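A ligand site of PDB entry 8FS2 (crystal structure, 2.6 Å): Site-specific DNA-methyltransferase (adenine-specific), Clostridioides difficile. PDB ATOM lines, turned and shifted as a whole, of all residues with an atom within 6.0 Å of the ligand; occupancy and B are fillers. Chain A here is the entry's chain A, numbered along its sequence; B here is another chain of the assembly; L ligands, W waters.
N7 of DA 8 of chain B lies within hydrogen-bond range of a nitrogen (N1) of the ligand (3.4 Å). O of Tyr 168 is in hydrogen-bond range of N3 of the ligand, at 2.8 Å. The side-chain carboxylate (OD1) of Asp 149 is in hydrogen-bond range of a nitrogen (N8) of the ligand, at 3.0 Å. A nitrogen (N6) of the ligand sits at hydrogen-bond distance from the backbone NH (N) of Ile 115 (3.4 Å). The backbone NH (N) of Ser 150 lies within hydrogen-bond range of a nitrogen (N7) of the ligand (3.0 Å). An oxygen (O3) of the ligand sits at hydrogen-bond distance from the side-chain carboxylate (OD1) of Asp 114 (2.5 Å).
The side-chain carboxylate of Asp 114 is in hydrogen-bond range of the backbone NH of Asp 116 (2.9 Å). The side-chain hydroxyl of Ser 150 sits at hydrogen-bond distance from the backbone carbonyl oxygen of Ile 61 (2.5 Å). O of Ala 113 sits close to N of Ser 62 (3.4 Å). OD1 of Asp 149 sits at hydrogen-bond distance from N of Leu 151 (2.8 Å). The side-chain hydroxyl (OH) of Tyr 168 lies within hydrogen-bond range of the side-chain amide oxygen (OD1) of Asn 165 (2.8 Å). N1 of DA 8 of chain B lies within hydrogen-bond range of ND2 of Asn 165 (3.2 Å). N7 of DA 8 of chain B sits at hydrogen-bond distance from N of Tyr 168, at 3.1 Å. The backbone carbonyl oxygen (O) of Asp 114 lies within hydrogen-bond range of the backbone NH (N) of Cys 148 (3.0 Å).
The backbone nitrogen (N) of Pro 167 sits close to a sulfur (S1) of the ligand. Merely in contact with the ligand: Ser 62 (3.3 Å), Tyr 178 (3.3 Å), Phe 200 (3.5 Å), Leu 196 (3.6 Å), Ile 169 (3.6 Å), Glu 175 (3.6 Å), Cys 148 (3.7 Å), Asp 116 (3.7 Å), Gly 64 (3.8 Å), Ile 61 (3.8 Å) and Tyr 30 (3.8 Å). Hydrophobic or aromatic side chains that line the ligand: Tyr 30, Ile 115, Pro 167, Ile 169, Tyr 178, Leu 196 and Phe 200. Of the 26 residues printed, 18 come within 4 Å of the ligand. The nearest printed residue that does not touch the ligand is Pro 166 (4.1 Å).
Water W1 lies within hydrogen-bond range of O of Tyr 168 (2.8 Å) and N3 of the ligand (2.9 Å).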
ATOM      1  N   TYR A  30      36.467 -12.349   9.463  1.00  0.00           N
ATOM      2  CA  TYR A  30      36.525 -11.270  10.444  1.00  0.00           C
ATOM      3  C   TYR A  30      37.421 -11.639  11.635  1.00  0.00           C
ATOM      4  O   TYR A  30      37.625 -10.835  12.544  1.00  0.00           O
ATOM      5  CB  TYR A  30      35.127 -10.895  10.940  1.00  0.00           C
ATOM      6  CG  TYR A  30      34.159 -10.532   9.833  1.00  0.00           C
ATOM      7  CD1 TYR A  30      34.387  -9.444   9.020  1.00  0.00           C
ATOM      8  CD2 TYR A  30      33.016 -11.295   9.609  1.00  0.00           C
ATOM      9  CE1 TYR A  30      33.503  -9.112   7.994  1.00  0.00           C
ATOM     10  CE2 TYR A  30      32.120 -10.977   8.597  1.00  0.00           C
ATOM     11  CZ  TYR A  30      32.370  -9.880   7.790  1.00  0.00           C
ATOM     12  OH  TYR A  30      31.503  -9.542   6.778  1.00  0.00           O
ATOM     13  N   ILE A  61      34.717  -5.259  23.782  1.00  0.00           N
ATOM     14  CA  ILE A  61      33.338  -4.829  23.621  1.00  0.00           C
ATOM     15  C   ILE A  61      32.655  -5.446  22.404  1.00  0.00           C
ATOM     16  O   ILE A  61      31.428  -5.309  22.247  1.00  0.00           O
ATOM     17  CB  ILE A  61      33.380  -3.296  23.592  1.00  0.00           C
ATOM     18  CG1 ILE A  61      32.531  -2.722  24.717  1.00  0.00           C
ATOM     19  CG2 ILE A  61      32.963  -2.738  22.267  1.00  0.00           C
ATOM     20  CD1 ILE A  61      32.671  -1.231  24.818  1.00  0.00           C
ATOM     21  N   SER A  62      33.394  -6.105  21.534  1.00  0.00           N
ATOM     22  CA  SER A  62      32.831  -6.896  20.435  1.00  0.00           C
ATOM     23  C   SER A  62      33.616  -8.196  20.358  1.00  0.00           C
ATOM     24  O   SER A  62      34.185  -8.545  19.322  1.00  0.00           O
ATOM     25  CB  SER A  62      32.839  -6.120  19.130  1.00  0.00           C
ATOM     26  OG  SER A  62      34.123  -5.593  18.881  1.00  0.00           O
ATOM     27  N   CYS A  63      33.701  -8.893  21.483  1.00  0.00           N
ATOM     28  CA  CYS A  63      34.680  -9.955  21.687  1.00  0.00           C
ATOM     29  C   CYS A  63      34.494 -11.144  20.752  1.00  0.00           C
ATOM     30  O   CYS A  63      35.451 -11.898  20.546  1.00  0.00           O
ATOM     31  CB  CYS A  63      34.615 -10.433  23.136  1.00  0.00           C
ATOM     32  SG  CYS A  63      33.000 -11.049  23.600  1.00  0.00           S
ATOM     33  N   GLY A  64      33.304 -11.337  20.190  1.00  0.00           N
ATOM     34  CA  GLY A  64      33.115 -12.459  19.279  1.00  0.00           C
ATOM     35  C   GLY A  64      33.402 -13.789  19.948  1.00  0.00           C
ATOM     36  O   GLY A  64      32.963 -14.048  21.073  1.00  0.00           O
ATOM     37  N   CYS A  65      34.154 -14.651  19.250  1.00  0.00           N
ATOM     38  CA  CYS A  65      34.526 -15.941  19.827  1.00  0.00           C
ATOM     39  C   CYS A  65      35.645 -15.839  20.849  1.00  0.00           C
ATOM     40  O   CYS A  65      36.002 -16.852  21.470  1.00  0.00           O
ATOM     41  CB  CYS A  65      34.916 -16.928  18.731  1.00  0.00           C
ATOM     42  SG  CYS A  65      33.503 -17.685  17.927  1.00  0.00           S
ATOM     43  N   ALA A 113      31.645  -8.449  25.688  1.00  0.00           N
ATOM     44  CA  ALA A 113      30.285  -8.149  25.237  1.00  0.00           C
ATOM     45  C   ALA A 113      30.176  -8.448  23.754  1.00  0.00           C
ATOM     46  O   ALA A 113      31.117  -8.207  23.001  1.00  0.00           O
ATOM     47  CB  ALA A 113      29.911  -6.684  25.479  1.00  0.00           C
ATOM     48  N   ASP A 114      29.010  -8.942  23.339  1.00  0.00           N
ATOM     49  CA  ASP A 114      28.754  -9.211  21.930  1.00  0.00           C
ATOM     50  C   ASP A 114      27.263  -9.446  21.728  1.00  0.00           C
ATOM     51  O   ASP A 114      26.589  -9.964  22.625  1.00  0.00           O
ATOM     52  CB  ASP A 114      29.554 -10.419  21.438  1.00  0.00           C
ATOM     53  CG  ASP A 114      29.755 -10.405  19.934  1.00  0.00           C
ATOM     54  OD1 ASP A 114      28.739 -10.453  19.202  1.00  0.00           O
ATOM     55  OD2 ASP A 114      30.925 -10.305  19.502  1.00  0.00           O
ATOM     56  N   ILE A 115      26.756  -9.072  20.550  1.00  0.00           N
ATOM     57  CA  ILE A 115      25.338  -9.300  20.265  1.00  0.00           C
ATOM     58  C   ILE A 115      25.032 -10.743  19.886  1.00  0.00           C
ATOM     59  O   ILE A 115      23.887 -11.166  20.020  1.00  0.00           O
ATOM     60  CB  ILE A 115      24.815  -8.402  19.130  1.00  0.00           C
ATOM     61  CG1 ILE A 115      25.834  -8.294  18.004  1.00  0.00           C
ATOM     62  CG2 ILE A 115      24.377  -7.027  19.648  1.00  0.00           C
ATOM     63  CD1 ILE A 115      25.323  -7.557  16.808  1.00  0.00           C
ATOM     64  N   ASP A 116      26.029 -11.503  19.430  1.00  0.00           N
ATOM     65  CA  ASP A 116      25.817 -12.880  18.970  1.00  0.00           C
ATOM     66  C   ASP A 116      25.934 -13.828  20.157  1.00  0.00           C
ATOM     67  O   ASP A 116      27.041 -14.105  20.639  1.00  0.00           O
ATOM     68  CB  ASP A 116      26.838 -13.234  17.891  1.00  0.00           C
ATOM     69  CG  ASP A 116      26.634 -14.642  17.342  1.00  0.00           C
ATOM     70  OD1 ASP A 116      25.586 -15.269  17.634  1.00  0.00           O
ATOM     71  OD2 ASP A 116      27.538 -15.115  16.622  1.00  0.00           O
ATOM     72  N   ALA A 119      28.220 -16.838  19.759  1.00  0.00           N
ATOM     73  CA  ALA A 119      29.623 -16.528  19.999  1.00  0.00           C
ATOM     74  C   ALA A 119      29.928 -16.473  21.491  1.00  0.00           C
ATOM     75  O   ALA A 119      30.939 -17.019  21.948  1.00  0.00           O
ATOM     76  CB  ALA A 119      29.980 -15.209  19.329  1.00  0.00           C
ATOM     77  N   CYS A 148      24.668  -8.509  24.414  1.00  0.00           N
ATOM     78  CA  CYS A 148      23.961  -7.242  24.354  1.00  0.00           C
ATOM     79  C   CYS A 148      24.535  -6.403  23.231  1.00  0.00           C
ATOM     80  O   CYS A 148      25.566  -6.742  22.631  1.00  0.00           O
ATOM     81  CB  CYS A 148      24.094  -6.466  25.671  1.00  0.00           C
ATOM     82  SG  CYS A 148      25.783  -5.836  25.911  1.00  0.00           S
ATOM     83  N   ASP A 149      23.875  -5.275  22.963  1.00  0.00           N
ATOM     84  CA  ASP A 149      24.411  -4.218  22.109  1.00  0.00           C
ATOM     85  C   ASP A 149      25.321  -3.350  22.951  1.00  0.00           C
ATOM     86  O   ASP A 149      24.850  -2.633  23.844  1.00  0.00           O
ATOM     87  CB  ASP A 149      23.270  -3.400  21.508  1.00  0.00           C
ATOM     88  CG  ASP A 149      23.750  -2.352  20.521  1.00  0.00           C
ATOM     89  OD1 ASP A 149      24.932  -1.932  20.579  1.00  0.00           O
ATOM     90  OD2 ASP A 149      22.932  -1.923  19.691  1.00  0.00           O
ATOM     91  N   SER A 150      26.622  -3.380  22.667  1.00  0.00           N
ATOM     92  CA  SER A 150      27.564  -2.621  23.486  1.00  0.00           C
ATOM     93  C   SER A 150      27.268  -1.127  23.451  1.00  0.00           C
ATOM     94  O   SER A 150      27.535  -0.424  24.437  1.00  0.00           O
ATOM     95  CB  SER A 150      28.995  -2.892  23.023  1.00  0.00           C
ATOM     96  OG  SER A 150      29.330  -4.249  23.216  1.00  0.00           O
ATOM     97  N   LEU A 151      26.722  -0.624  22.346  1.00  0.00           N
ATOM     98  CA  LEU A 151      26.393   0.787  22.231  1.00  0.00           C
ATOM     99  C   LEU A 151      25.146   1.176  23.008  1.00  0.00           C
ATOM    100  O   LEU A 151      24.873   2.361  23.155  1.00  0.00           O
ATOM    101  CB  LEU A 151      26.247   1.174  20.757  1.00  0.00           C
ATOM    102  CG  LEU A 151      27.478   0.931  19.884  1.00  0.00           C
ATOM    103  CD1 LEU A 151      27.247   1.494  18.508  1.00  0.00           C
ATOM    104  CD2 LEU A 151      28.745   1.513  20.531  1.00  0.00           C
ATOM    105  N   ASN A 165      38.448  -5.666  18.119  1.00  0.00           N
ATOM    106  CA  ASN A 165      38.214  -5.333  16.720  1.00  0.00           C
ATOM    107  C   ASN A 165      36.718  -5.079  16.536  1.00  0.00           C
ATOM    108  O   ASN A 165      35.931  -6.035  16.388  1.00  0.00           O
ATOM    109  CB  ASN A 165      38.707  -6.451  15.827  1.00  0.00           C
ATOM    110  CG  ASN A 165      38.456  -6.195  14.362  1.00  0.00           C
ATOM    111  OD1 ASN A 165      38.218  -5.060  13.956  1.00  0.00           O
ATOM    112  ND2 ASN A 165      38.547  -7.235  13.551  1.00  0.00           N
ATOM    113  N   PRO A 166      36.278  -3.813  16.537  1.00  0.00           N
ATOM    114  CA  PRO A 166      34.831  -3.509  16.489  1.00  0.00           C
ATOM    115  C   PRO A 166      34.246  -3.787  15.122  1.00  0.00           C
ATOM    116  O   PRO A 166      34.980  -3.980  14.140  1.00  0.00           O
ATOM    117  CB  PRO A 166      34.796  -1.997  16.791  1.00  0.00           C
ATOM    118  CG  PRO A 166      36.089  -1.493  16.279  1.00  0.00           C
ATOM    119  CD  PRO A 166      37.104  -2.598  16.577  1.00  0.00           C
ATOM    120  N   PRO A 167      32.913  -3.822  15.015  1.00  0.00           N
ATOM    121  CA  PRO A 167      32.278  -3.977  13.699  1.00  0.00           C
ATOM    122  C   PRO A 167      32.389  -2.708  12.873  1.00  0.00           C
ATOM    123  O   PRO A 167      32.317  -1.593  13.398  1.00  0.00           O
ATOM    124  CB  PRO A 167      30.822  -4.274  14.043  1.00  0.00           C
ATOM    125  CG  PRO A 167      30.629  -3.635  15.380  1.00  0.00           C
ATOM    126  CD  PRO A 167      31.923  -3.808  16.099  1.00  0.00           C
ATOM    127  N   TYR A 168      32.555  -2.889  11.557  1.00  0.00           N
ATOM    128  CA  TYR A 168      32.581  -1.791  10.595  1.00  0.00           C
ATOM    129  C   TYR A 168      31.323  -1.885   9.736  1.00  0.00           C
ATOM    130  O   TYR A 168      31.144  -2.860   8.989  1.00  0.00           O
ATOM    131  CB  TYR A 168      33.803  -1.837   9.666  1.00  0.00           C
ATOM    132  CG  TYR A 168      35.129  -2.416  10.176  1.00  0.00           C
ATOM    133  CD1 TYR A 168      35.483  -2.392  11.520  1.00  0.00           C
ATOM    134  CD2 TYR A 168      36.041  -2.960   9.269  1.00  0.00           C
ATOM    135  CE1 TYR A 168      36.720  -2.921  11.960  1.00  0.00           C
ATOM    136  CE2 TYR A 168      37.262  -3.476   9.700  1.00  0.00           C
ATOM    137  CZ  TYR A 168      37.601  -3.461  11.044  1.00  0.00           C
ATOM    138  OH  TYR A 168      38.820  -3.974  11.462  1.00  0.00           O
ATOM    139  N   ILE A 169      30.441  -0.893   9.831  1.00  0.00           N
ATOM    140  CA  ILE A 169      29.243  -0.860   8.991  1.00  0.00           C
ATOM    141  C   ILE A 169      29.057   0.557   8.466  1.00  0.00           C
ATOM    142  O   ILE A 169      28.891   1.493   9.251  1.00  0.00           O
ATOM    143  CB  ILE A 169      27.986  -1.304   9.733  1.00  0.00           C
ATOM    144  CG1 ILE A 169      28.192  -2.698  10.341  1.00  0.00           C
ATOM    145  CG2 ILE A 169      26.819  -1.315   8.768  1.00  0.00           C
ATOM    146  CD1 ILE A 169      27.050  -3.177  11.174  1.00  0.00           C
ATOM    147  N   LEU A 174      23.983   0.037   7.044  1.00  0.00           N
ATOM    148  CA  LEU A 174      23.464   0.172   8.389  1.00  0.00           C
ATOM    149  C   LEU A 174      21.949   0.340   8.365  1.00  0.00           C
ATOM    150  O   LEU A 174      21.402   1.068   7.532  1.00  0.00           O
ATOM    151  CB  LEU A 174      24.100   1.367   9.093  1.00  0.00           C
ATOM    152  CG  LEU A 174      23.987   1.409  10.610  1.00  0.00           C
ATOM    153  CD1 LEU A 174      24.336   0.050  11.219  1.00  0.00           C
ATOM    154  CD2 LEU A 174      24.925   2.470  11.133  1.00  0.00           C
ATOM    155  N   GLU A 175      21.270  -0.355   9.273  1.00  0.00           N
ATOM    156  CA  GLU A 175      19.812  -0.300   9.331  1.00  0.00           C
ATOM    157  C   GLU A 175      19.336   1.099   9.699  1.00  0.00           C
ATOM    158  O   GLU A 175      19.876   1.740  10.598  1.00  0.00           O
ATOM    159  CB  GLU A 175      19.309  -1.334  10.354  1.00  0.00           C
ATOM    160  CG  GLU A 175      17.844  -1.240  10.694  1.00  0.00           C
ATOM    161  CD  GLU A 175      17.452  -2.212  11.787  1.00  0.00           C
ATOM    162  OE1 GLU A 175      18.239  -3.136  12.089  1.00  0.00           O
ATOM    163  OE2 GLU A 175      16.338  -2.056  12.350  1.00  0.00           O
ATOM    164  N   TYR A 178      18.190   1.830  13.225  1.00  0.00           N
ATOM    165  CA  TYR A 178      19.338   1.920  14.115  1.00  0.00           C
ATOM    166  C   TYR A 178      20.095   3.236  13.947  1.00  0.00           C
ATOM    167  O   TYR A 178      20.639   3.769  14.916  1.00  0.00           O
ATOM    168  CB  TYR A 178      20.282   0.736  13.863  1.00  0.00           C
ATOM    169  CG  TYR A 178      21.279   0.545  14.977  1.00  0.00           C
ATOM    170  CD1 TYR A 178      20.929  -0.181  16.112  1.00  0.00           C
ATOM    171  CD2 TYR A 178      22.549   1.093  14.911  1.00  0.00           C
ATOM    172  CE1 TYR A 178      21.814  -0.350  17.146  1.00  0.00           C
ATOM    173  CE2 TYR A 178      23.448   0.934  15.944  1.00  0.00           C
ATOM    174  CZ  TYR A 178      23.073   0.202  17.060  1.00  0.00           C
ATOM    175  OH  TYR A 178      23.958   0.023  18.092  1.00  0.00           O
ATOM    176  N   LEU A 196      29.757   2.974  11.702  1.00  0.00           N
ATOM    177  CA  LEU A 196      29.430   2.449  13.034  1.00  0.00           C
ATOM    178  C   LEU A 196      30.653   2.401  13.939  1.00  0.00           C
ATOM    179  O   LEU A 196      30.555   2.675  15.148  1.00  0.00           O
ATOM    180  CB  LEU A 196      28.812   1.054  12.898  1.00  0.00           C
ATOM    181  CG  LEU A 196      28.467   0.350  14.207  1.00  0.00           C
ATOM    182  CD1 LEU A 196      27.390   1.104  14.931  1.00  0.00           C
ATOM    183  CD2 LEU A 196      28.080  -1.066  13.949  1.00  0.00           C
ATOM    184  N   PHE A 200      31.949   3.007  18.346  1.00  0.00           N
ATOM    185  CA  PHE A 200      32.708   2.154  19.249  1.00  0.00           C
ATOM    186  C   PHE A 200      33.917   2.881  19.806  1.00  0.00           C
ATOM    187  O   PHE A 200      34.231   2.758  20.991  1.00  0.00           O
ATOM    188  CB  PHE A 200      33.115   0.865  18.536  1.00  0.00           C
ATOM    189  CG  PHE A 200      32.034  -0.172  18.518  1.00  0.00           C
ATOM    190  CD1 PHE A 200      30.960  -0.064  17.647  1.00  0.00           C
ATOM    191  CD2 PHE A 200      32.079  -1.251  19.386  1.00  0.00           C
ATOM    192  CE1 PHE A 200      29.952  -1.014  17.639  1.00  0.00           C
ATOM    193  CE2 PHE A 200      31.079  -2.212  19.381  1.00  0.00           C
ATOM    194  CZ  PHE A 200      30.003  -2.091  18.498  1.00  0.00           C
ATOM    195  P    DA B   8      32.374  -0.941   3.108  1.00  0.00           P
ATOM    196  OP1  DA B   8      31.419  -1.732   2.298  1.00  0.00           O
ATOM    197  OP2  DA B   8      31.897  -0.112   4.233  1.00  0.00           O
ATOM    198  O5'  DA B   8      33.541  -1.878   3.642  1.00  0.00           O
ATOM    199  C5'  DA B   8      33.412  -2.549   4.865  1.00  0.00           C
ATOM    200  C4'  DA B   8      34.272  -3.786   4.857  1.00  0.00           C
ATOM    201  O4'  DA B   8      34.809  -4.040   6.182  1.00  0.00           O
ATOM    202  C3'  DA B   8      33.564  -5.060   4.425  1.00  0.00           C
ATOM    203  O3'  DA B   8      34.430  -5.802   3.634  1.00  0.00           O
ATOM    204  C2'  DA B   8      33.310  -5.763   5.764  1.00  0.00           C
ATOM    205  C1'  DA B   8      34.572  -5.390   6.518  1.00  0.00           C
ATOM    206  N9   DA B   8      34.470  -5.528   7.970  1.00  0.00           N
ATOM    207  C8   DA B   8      33.413  -5.181   8.766  1.00  0.00           C
ATOM    208  N7   DA B   8      33.605  -5.422  10.039  1.00  0.00           N
ATOM    209  C5   DA B   8      34.890  -5.959  10.095  1.00  0.00           C
ATOM    210  C6   DA B   8      35.702  -6.431  11.165  1.00  0.00           C
ATOM    211  N6   DA B   8      35.316  -6.430  12.445  1.00  0.00           N
ATOM    212  N1   DA B   8      36.930  -6.906  10.863  1.00  0.00           N
ATOM    213  C2   DA B   8      37.317  -6.908   9.584  1.00  0.00           C
ATOM    214  N3   DA B   8      36.652  -6.498   8.498  1.00  0.00           N
ATOM    215  C4   DA B   8      35.434  -6.038   8.817  1.00  0.00           C
HETATM  216  C1  LIG L   1      30.751  -9.925  15.969  1.00  0.00           C
HETATM  217  C2  LIG L   1      29.411  -9.195  16.200  1.00  0.00           C
HETATM  218  C3  LIG L   1      31.786  -8.983  16.603  1.00  0.00           C
HETATM  219  C4  LIG L   1      32.979  -8.773  15.678  1.00  0.00           C
HETATM  220  C5  LIG L   1      32.165  -8.379  12.997  1.00  0.00           C
HETATM  221  C6  LIG L   1      26.505  -7.296  11.331  1.00  0.00           C
HETATM  222  C7  LIG L   1      25.565  -9.206  13.483  1.00  0.00           C
HETATM  223  C8  LIG L   1      24.635  -8.603  12.440  1.00  0.00           C
HETATM  224  C9  LIG L   1      25.382  -8.313  11.134  1.00  0.00           C
HETATM  225  C10 LIG L   1      30.891  -7.857  12.364  1.00  0.00           C
HETATM  226  C11 LIG L   1      30.717  -8.265  10.924  1.00  0.00           C
HETATM  227  C12 LIG L   1      29.656  -6.409   9.529  1.00  0.00           C
HETATM  228  C13 LIG L   1      27.767  -7.729  10.608  1.00  0.00           C
HETATM  229  C14 LIG L   1      26.758  -7.095  12.813  1.00  0.00           C
HETATM  230  C15 LIG L   1      26.870  -8.424  13.554  1.00  0.00           C
HETATM  231  C16 LIG L   1      29.791  -8.106  17.184  1.00  0.00           C
HETATM  232  C17 LIG L   1      28.454  -6.253  16.073  1.00  0.00           C
HETATM  233  C18 LIG L   1      27.759  -5.148  17.736  1.00  0.00           C
HETATM  234  C19 LIG L   1      28.479  -6.211  18.252  1.00  0.00           C
HETATM  235  C20 LIG L   1      28.145  -5.541  20.337  1.00  0.00           C
HETATM  236  C21 LIG L   1      27.202  -4.245  18.677  1.00  0.00           C
HETATM  237  C22 LIG L   1      25.301  -3.377  17.377  1.00  0.00           C
HETATM  238  C23 LIG L   1      25.634  -2.760  16.043  1.00  0.00           C
HETATM  239  C24 LIG L   1      24.393  -2.285  15.297  1.00  0.00           C
HETATM  240  C25 LIG L   1      23.517  -3.315  14.625  1.00  0.00           C
HETATM  241  C26 LIG L   1      24.055  -4.509  14.156  1.00  0.00           C
HETATM  242  C27 LIG L   1      23.257  -5.427  13.475  1.00  0.00           C
HETATM  243  C28 LIG L   1      21.915  -5.153  13.272  1.00  0.00           C
HETATM  244  C29 LIG L   1      21.376  -3.978  13.737  1.00  0.00           C
HETATM  245  C30 LIG L   1      22.166  -3.059  14.412  1.00  0.00           C
HETATM  246  N1  LIG L   1      30.700  -7.117  10.016  1.00  0.00           N
HETATM  247  N2  LIG L   1      28.361  -6.663   9.798  1.00  0.00           N
HETATM  248  N3  LIG L   1      29.965  -5.439   8.727  1.00  0.00           N
HETATM  249  N4  LIG L   1      28.935  -6.926  17.171  1.00  0.00           N
HETATM  250  N5  LIG L   1      27.742  -5.194  16.348  1.00  0.00           N
HETATM  251  N6  LIG L   1      28.712  -6.470  19.550  1.00  0.00           N
HETATM  252  N7  LIG L   1      27.416  -4.476  19.993  1.00  0.00           N
HETATM  253  N8  LIG L   1      26.381  -3.240  18.340  1.00  0.00           N
HETATM  254  O1  LIG L   1      31.101  -7.729  16.823  1.00  0.00           O
HETATM  255  O2  LIG L   1      30.831 -11.228  16.552  1.00  0.00           O
HETATM  256  O3  LIG L   1      28.419 -10.015  16.798  1.00  0.00           O
HETATM  257  S1  LIG L   1      32.590  -7.469  14.498  1.00  0.00           S
HETATM  258  O   HOH W   1      30.294  -3.659   6.421  1.00  0.00           O
